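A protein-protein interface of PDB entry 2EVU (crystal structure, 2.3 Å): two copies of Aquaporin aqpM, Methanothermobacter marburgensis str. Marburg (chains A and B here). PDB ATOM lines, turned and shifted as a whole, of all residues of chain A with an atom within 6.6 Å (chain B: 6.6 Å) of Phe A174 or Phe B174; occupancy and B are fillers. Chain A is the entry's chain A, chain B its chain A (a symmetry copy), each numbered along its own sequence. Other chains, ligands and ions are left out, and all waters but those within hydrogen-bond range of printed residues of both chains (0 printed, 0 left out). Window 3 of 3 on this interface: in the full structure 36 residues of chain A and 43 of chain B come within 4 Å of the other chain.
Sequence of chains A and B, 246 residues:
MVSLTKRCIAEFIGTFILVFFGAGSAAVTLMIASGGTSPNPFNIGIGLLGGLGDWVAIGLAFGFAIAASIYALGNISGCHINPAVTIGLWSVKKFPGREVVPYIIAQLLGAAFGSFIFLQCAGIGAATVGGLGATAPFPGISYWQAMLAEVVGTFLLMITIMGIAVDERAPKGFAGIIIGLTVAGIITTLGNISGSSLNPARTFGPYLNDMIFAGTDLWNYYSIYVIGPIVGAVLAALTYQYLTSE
The side-chain hydroxyl of Tyr A71 sits at hydrogen-bond distance from the backbone carbonyl oxygen of Gly A173, at 2.5 Å.
OH of Tyr A71 lies within hydrogen-bond range of N of Ile A177.
Ile B164 touches Tyr A71 (CD1 to CD1, 3.6 Å).
Tyr A71 touches Phe B174 (OH to CD1, 3.9 Å).
Ile B178 touches Tyr A71.
Gly A173 touches Pro B171.
Phe B174 touches Gly A173 (CE1 to O, 3.3 Å).
Phe A174 touches Phe B174 (CE2 to CZ, 3.7 Å).
Of the printed residues of chain B, Tyr A71 touches Ile B164, Phe B174 and Ile B178.
Printed residues of chain B within 4 Å of Gly A173: Pro B171 and Phe B174.
Phe A174 touches just one residue of chain B: Phe B174 (3.7 Å).
Ile A179 touches none of the printed residues of chain B.
Of the printed residues of chain A, Ile B164 touches Tyr A71.
Of the printed residues of chain A, Pro B171 touches Gly A173.
Of the printed residues of chain A, Phe B174 touches Tyr A71, Gly A173 and Phe A174.
Ile B177 touches none of the printed residues of chain A.
Of the printed residues of chain A, Ile B178 touches Tyr A71 (3.4 Å).
The nearest printed residue of chain A that does not touch Phe B174 is Lys A172 (4.001 Å).
Hydrophobic or aromatic side chains of chain B that line the printed part of chain A: Ile B164, Pro B171, Phe B174 and Ile B178.
Of the 12 printed residues of chain A, 3 touch a printed residue of chain B.
Printed residues of chain A that touch a printed residue of chain B: Tyr A71, Gly A173 and Phe A174.
Hydrophobic or aromatic side chains of chain A that line the printed part of chain B: Tyr A71 and Phe A174.
Among the printed residues, 6 pairs touch across the chains.
Among the printed residues, no Asp or Glu carboxylate lies within 4 Å of a Lys or Arg side-chain nitrogen of the other chain.
Tyr A71 touches Phe B174, but with the chains exchanged Phe A174 does not touch Tyr B71 (9.9 Å).
Tyr A71 touches Ile B178, but with the chains exchanged Ile A178 does not touch Tyr B71 (12.8 Å).
Gly A173 touches Pro B171, but with the chains exchanged Pro A171 does not touch Gly B173 (11.9 Å).
Gly A173 touches Phe B174, but with the chains exchanged Phe A174 does not touch Gly B173 (8.7 Å).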
ATOM      1  N   TYR A  71      10.317   0.146 -29.717  1.00  0.00           N
ATOM      2  CA  TYR A  71       9.369  -0.013 -28.622  1.00  0.00           C
ATOM      3  C   TYR A  71       9.032  -1.482 -28.424  1.00  0.00           C
ATOM      4  O   TYR A  71       8.737  -1.915 -27.314  1.00  0.00           O
ATOM      5  CB  TYR A  71       8.085   0.786 -28.891  1.00  0.00           C
ATOM      6  CG  TYR A  71       8.255   2.267 -28.660  1.00  0.00           C
ATOM      7  CD1 TYR A  71       8.440   2.777 -27.371  1.00  0.00           C
ATOM      8  CD2 TYR A  71       8.303   3.159 -29.734  1.00  0.00           C
ATOM      9  CE1 TYR A  71       8.678   4.138 -27.163  1.00  0.00           C
ATOM     10  CE2 TYR A  71       8.543   4.512 -29.537  1.00  0.00           C
ATOM     11  CZ  TYR A  71       8.733   4.994 -28.255  1.00  0.00           C
ATOM     12  OH  TYR A  71       9.016   6.327 -28.076  1.00  0.00           O
ATOM     13  N   ILE A 164      19.745  10.583 -26.420  1.00  0.00           N
ATOM     14  CA  ILE A 164      18.452  10.143 -25.941  1.00  0.00           C
ATOM     15  C   ILE A 164      18.288   8.681 -25.514  1.00  0.00           C
ATOM     16  O   ILE A 164      17.299   8.334 -24.872  1.00  0.00           O
ATOM     17  CB  ILE A 164      17.365  10.505 -26.974  1.00  0.00           C
ATOM     18  CG1 ILE A 164      16.026  10.690 -26.255  1.00  0.00           C
ATOM     19  CG2 ILE A 164      17.285   9.432 -28.062  1.00  0.00           C
ATOM     20  CD1 ILE A 164      14.936  11.144 -27.145  1.00  0.00           C
ATOM     21  N   ALA A 170      18.508  11.038 -20.193  1.00  0.00           N
ATOM     22  CA  ALA A 170      17.506  11.079 -21.251  1.00  0.00           C
ATOM     23  C   ALA A 170      16.081  10.871 -20.743  1.00  0.00           C
ATOM     24  O   ALA A 170      15.851  10.140 -19.784  1.00  0.00           O
ATOM     25  CB  ALA A 170      17.838  10.032 -22.316  1.00  0.00           C
ATOM     26  N   PRO A 171      15.102  11.524 -21.386  1.00  0.00           N
ATOM     27  CA  PRO A 171      13.695  11.398 -20.994  1.00  0.00           C
ATOM     28  C   PRO A 171      13.207   9.991 -21.344  1.00  0.00           C
ATOM     29  O   PRO A 171      13.225   9.595 -22.507  1.00  0.00           O
ATOM     30  CB  PRO A 171      12.997  12.460 -21.842  1.00  0.00           C
ATOM     31  CG  PRO A 171      14.095  13.409 -22.212  1.00  0.00           C
ATOM     32  CD  PRO A 171      15.255  12.507 -22.467  1.00  0.00           C
ATOM     33  N   LYS A 172      12.761   9.240 -20.348  1.00  0.00           N
ATOM     34  CA  LYS A 172      12.300   7.881 -20.602  1.00  0.00           C
ATOM     35  C   LYS A 172      11.091   7.752 -21.518  1.00  0.00           C
ATOM     36  O   LYS A 172      10.097   8.466 -21.372  1.00  0.00           O
ATOM     37  CB  LYS A 172      12.037   7.169 -19.274  1.00  0.00           C
ATOM     38  CG  LYS A 172      13.328   6.750 -18.599  1.00  0.00           C
ATOM     39  CD  LYS A 172      13.109   6.144 -17.238  1.00  0.00           C
ATOM     40  CE  LYS A 172      14.419   5.566 -16.719  1.00  0.00           C
ATOM     41  NZ  LYS A 172      15.534   6.561 -16.810  1.00  0.00           N
ATOM     42  N   GLY A 173      11.199   6.837 -22.477  1.00  0.00           N
ATOM     43  CA  GLY A 173      10.116   6.589 -23.412  1.00  0.00           C
ATOM     44  C   GLY A 173      10.200   7.328 -24.735  1.00  0.00           C
ATOM     45  O   GLY A 173       9.481   6.984 -25.669  1.00  0.00           O
ATOM     46  N   PHE A 174      11.076   8.328 -24.824  1.00  0.00           N
ATOM     47  CA  PHE A 174      11.219   9.124 -26.043  1.00  0.00           C
ATOM     48  C   PHE A 174      12.204   8.592 -27.083  1.00  0.00           C
ATOM     49  O   PHE A 174      12.121   8.943 -28.261  1.00  0.00           O
ATOM     50  CB  PHE A 174      11.617  10.567 -25.687  1.00  0.00           C
ATOM     51  CG  PHE A 174      10.497  11.383 -25.104  1.00  0.00           C
ATOM     52  CD1 PHE A 174       9.686  12.161 -25.923  1.00  0.00           C
ATOM     53  CD2 PHE A 174      10.242  11.364 -23.733  1.00  0.00           C
ATOM     54  CE1 PHE A 174       8.624  12.915 -25.388  1.00  0.00           C
ATOM     55  CE2 PHE A 174       9.189  12.112 -23.188  1.00  0.00           C
ATOM     56  CZ  PHE A 174       8.378  12.888 -24.020  1.00  0.00           C
ATOM     57  N   ALA A 175      13.137   7.754 -26.663  1.00  0.00           N
ATOM     58  CA  ALA A 175      14.139   7.238 -27.592  1.00  0.00           C
ATOM     59  C   ALA A 175      13.559   6.671 -28.884  1.00  0.00           C
ATOM     60  O   ALA A 175      13.975   7.053 -29.980  1.00  0.00           O
ATOM     61  CB  ALA A 175      15.001   6.195 -26.905  1.00  0.00           C
ATOM     62  N   GLY A 176      12.599   5.765 -28.757  1.00  0.00           N
ATOM     63  CA  GLY A 176      12.006   5.156 -29.935  1.00  0.00           C
ATOM     64  C   GLY A 176      11.501   6.109 -31.009  1.00  0.00           C
ATOM     65  O   GLY A 176      11.938   6.045 -32.164  1.00  0.00           O
ATOM     66  N   ILE A 177      10.577   6.993 -30.639  1.00  0.00           N
ATOM     67  CA  ILE A 177      10.016   7.919 -31.604  1.00  0.00           C
ATOM     68  C   ILE A 177      11.034   8.946 -32.094  1.00  0.00           C
ATOM     69  O   ILE A 177      11.056   9.280 -33.284  1.00  0.00           O
ATOM     70  CB  ILE A 177       8.744   8.628 -31.030  1.00  0.00           C
ATOM     71  CG1 ILE A 177       8.071   9.464 -32.124  1.00  0.00           C
ATOM     72  CG2 ILE A 177       9.103   9.499 -29.834  1.00  0.00           C
ATOM     73  CD1 ILE A 177       7.649   8.642 -33.343  1.00  0.00           C
ATOM     74  N   ILE A 178      11.899   9.427 -31.203  1.00  0.00           N
ATOM     75  CA  ILE A 178      12.894  10.416 -31.603  1.00  0.00           C
ATOM     76  C   ILE A 178      13.909   9.840 -32.591  1.00  0.00           C
ATOM     77  O   ILE A 178      14.224  10.463 -33.610  1.00  0.00           O
ATOM     78  CB  ILE A 178      13.632  11.021 -30.364  1.00  0.00           C
ATOM     79  CG1 ILE A 178      12.611  11.700 -29.441  1.00  0.00           C
ATOM     80  CG2 ILE A 178      14.659  12.080 -30.809  1.00  0.00           C
ATOM     81  CD1 ILE A 178      11.736  12.725 -30.161  1.00  0.00           C
ATOM     82  N   ILE A 179      14.416   8.646 -32.301  1.00  0.00           N
ATOM     83  CA  ILE A 179      15.383   8.027 -33.183  1.00  0.00           C
ATOM     84  C   ILE A 179      14.736   7.836 -34.545  1.00  0.00           C
ATOM     85  O   ILE A 179      15.324   8.149 -35.580  1.00  0.00           O
ATOM     86  CB  ILE A 179      15.855   6.669 -32.605  1.00  0.00           C
ATOM     87  CG1 ILE A 179      16.660   6.912 -31.323  1.00  0.00           C
ATOM     88  CG2 ILE A 179      16.722   5.925 -33.619  1.00  0.00           C
ATOM     89  CD1 ILE A 179      16.941   5.641 -30.524  1.00  0.00           C
ATOM     90  N   TYR B  71      -6.494   7.230 -27.004  1.00  0.00           N
ATOM     91  CA  TYR B  71      -6.405   8.152 -25.880  1.00  0.00           C
ATOM     92  C   TYR B  71      -7.792   8.461 -25.339  1.00  0.00           C
ATOM     93  O   TYR B  71      -7.959   8.727 -24.152  1.00  0.00           O
ATOM     94  CB  TYR B  71      -5.705   9.455 -26.295  1.00  0.00           C
ATOM     95  CG  TYR B  71      -4.209   9.305 -26.417  1.00  0.00           C
ATOM     96  CD1 TYR B  71      -3.412   9.101 -25.285  1.00  0.00           C
ATOM     97  CD2 TYR B  71      -3.590   9.293 -27.669  1.00  0.00           C
ATOM     98  CE1 TYR B  71      -2.037   8.881 -25.404  1.00  0.00           C
ATOM     99  CE2 TYR B  71      -2.225   9.071 -27.796  1.00  0.00           C
ATOM    100  CZ  TYR B  71      -1.457   8.863 -26.666  1.00  0.00           C
ATOM    101  OH  TYR B  71      -0.116   8.598 -26.807  1.00  0.00           O
ATOM    102  N   ILE B 164       4.527  -2.092 -26.438  1.00  0.00           N
ATOM    103  CA  ILE B 164       4.195  -0.817 -25.840  1.00  0.00           C
ATOM    104  C   ILE B 164       2.870  -0.685 -25.082  1.00  0.00           C
ATOM    105  O   ILE B 164       2.670   0.284 -24.354  1.00  0.00           O
ATOM    106  CB  ILE B 164       4.296   0.298 -26.902  1.00  0.00           C
ATOM    107  CG1 ILE B 164       4.627   1.624 -26.214  1.00  0.00           C
ATOM    108  CG2 ILE B 164       2.999   0.382 -27.710  1.00  0.00           C
ATOM    109  CD1 ILE B 164       4.852   2.740 -27.158  1.00  0.00           C
ATOM    110  N   ALA B 170       6.398  -0.978 -20.457  1.00  0.00           N
ATOM    111  CA  ALA B 170       6.182   0.046 -21.472  1.00  0.00           C
ATOM    112  C   ALA B 170       6.081   1.457 -20.896  1.00  0.00           C
ATOM    113  O   ALA B 170       5.590   1.655 -19.788  1.00  0.00           O
ATOM    114  CB  ALA B 170       4.921  -0.280 -22.273  1.00  0.00           C
ATOM    115  N   PRO B 171       6.557   2.460 -21.649  1.00  0.00           N
ATOM    116  CA  PRO B 171       6.510   3.856 -21.204  1.00  0.00           C
ATOM    117  C   PRO B 171       5.054   4.328 -21.208  1.00  0.00           C
ATOM    118  O   PRO B 171       4.400   4.328 -22.247  1.00  0.00           O
ATOM    119  CB  PRO B 171       7.338   4.589 -22.258  1.00  0.00           C
ATOM    120  CG  PRO B 171       8.188   3.515 -22.863  1.00  0.00           C
ATOM    121  CD  PRO B 171       7.264   2.346 -22.932  1.00  0.00           C
ATOM    122  N   LYS B 172       4.549   4.741 -20.055  1.00  0.00           N
ATOM    123  CA  LYS B 172       3.164   5.186 -19.976  1.00  0.00           C
ATOM    124  C   LYS B 172       2.813   6.411 -20.808  1.00  0.00           C
ATOM    125  O   LYS B 172       3.530   7.413 -20.807  1.00  0.00           O
ATOM    126  CB  LYS B 172       2.776   5.409 -18.513  1.00  0.00           C
ATOM    127  CG  LYS B 172       2.539   4.097 -17.791  1.00  0.00           C
ATOM    128  CD  LYS B 172       2.262   4.278 -16.322  1.00  0.00           C
ATOM    129  CE  LYS B 172       1.835   2.948 -15.715  1.00  0.00           C
ATOM    130  NZ  LYS B 172       2.794   1.852 -16.060  1.00  0.00           N
ATOM    131  N   GLY B 173       1.701   6.308 -21.532  1.00  0.00           N
ATOM    132  CA  GLY B 173       1.231   7.405 -22.358  1.00  0.00           C
ATOM    133  C   GLY B 173       1.645   7.361 -23.817  1.00  0.00           C
ATOM    134  O   GLY B 173       1.086   8.094 -24.629  1.00  0.00           O
ATOM    135  N   PHE B 174       2.607   6.503 -24.157  1.00  0.00           N
ATOM    136  CA  PHE B 174       3.100   6.399 -25.530  1.00  0.00           C
ATOM    137  C   PHE B 174       2.353   5.428 -26.442  1.00  0.00           C
ATOM    138  O   PHE B 174       2.421   5.541 -27.667  1.00  0.00           O
ATOM    139  CB  PHE B 174       4.591   6.018 -25.527  1.00  0.00           C
ATOM    140  CG  PHE B 174       5.507   7.138 -25.121  1.00  0.00           C
ATOM    141  CD1 PHE B 174       6.065   7.978 -26.079  1.00  0.00           C
ATOM    142  CD2 PHE B 174       5.804   7.365 -23.778  1.00  0.00           C
ATOM    143  CE1 PHE B 174       6.911   9.041 -25.707  1.00  0.00           C
ATOM    144  CE2 PHE B 174       6.646   8.418 -23.396  1.00  0.00           C
ATOM    145  CZ  PHE B 174       7.199   9.259 -24.365  1.00  0.00           C
ATOM    146  N   ALA B 175       1.645   4.473 -25.862  1.00  0.00           N
ATOM    147  CA  ALA B 175       0.940   3.481 -26.670  1.00  0.00           C
ATOM    148  C   ALA B 175       0.082   4.079 -27.781  1.00  0.00           C
ATOM    149  O   ALA B 175       0.204   3.692 -28.945  1.00  0.00           O
ATOM    150  CB  ALA B 175       0.093   2.589 -25.781  1.00  0.00           C
ATOM    151  N   GLY B 176      -0.781   5.021 -27.425  1.00  0.00           N
ATOM    152  CA  GLY B 176      -1.653   5.628 -28.416  1.00  0.00           C
ATOM    153  C   GLY B 176      -0.980   6.171 -29.669  1.00  0.00           C
ATOM    154  O   GLY B 176      -1.305   5.757 -30.788  1.00  0.00           O
ATOM    155  N   ILE B 177      -0.045   7.101 -29.491  1.00  0.00           N
ATOM    156  CA  ILE B 177       0.627   7.698 -30.630  1.00  0.00           C
ATOM    157  C   ILE B 177       1.523   6.707 -31.369  1.00  0.00           C
ATOM    158  O   ILE B 177       1.573   6.715 -32.604  1.00  0.00           O
ATOM    159  CB  ILE B 177       1.435   8.969 -30.206  1.00  0.00           C
ATOM    160  CG1 ILE B 177       1.987   9.678 -31.447  1.00  0.00           C
ATOM    161  CG2 ILE B 177       2.563   8.599 -29.253  1.00  0.00           C
ATOM    162  CD1 ILE B 177       0.901  10.112 -32.432  1.00  0.00           C
ATOM    163  N   ILE B 178       2.207   5.832 -30.634  1.00  0.00           N
ATOM    164  CA  ILE B 178       3.087   4.861 -31.276  1.00  0.00           C
ATOM    165  C   ILE B 178       2.310   3.857 -32.128  1.00  0.00           C
ATOM    166  O   ILE B 178       2.683   3.575 -33.271  1.00  0.00           O
ATOM    167  CB  ILE B 178       3.972   4.107 -30.228  1.00  0.00           C
ATOM    168  CG1 ILE B 178       4.835   5.120 -29.463  1.00  0.00           C
ATOM    169  CG2 ILE B 178       4.910   3.107 -30.931  1.00  0.00           C
ATOM    170  CD1 ILE B 178       5.655   6.026 -30.381  1.00  0.00           C
ATOM    171  N   ILE B 179       1.221   3.325 -31.582  1.00  0.00           N
ATOM    172  CA  ILE B 179       0.426   2.367 -32.320  1.00  0.00           C
ATOM    173  C   ILE B 179      -0.083   3.039 -33.585  1.00  0.00           C
ATOM    174  O   ILE B 179      -0.012   2.478 -34.678  1.00  0.00           O
ATOM    175  CB  ILE B 179      -0.756   1.861 -31.455  1.00  0.00           C
ATOM    176  CG1 ILE B 179      -0.215   1.034 -30.283  1.00  0.00           C
ATOM    177  CG2 ILE B 179      -1.706   1.003 -32.290  1.00  0.00           C
ATOM    178  CD1 ILE B 179      -1.262   0.716 -29.219  1.00  0.00           C
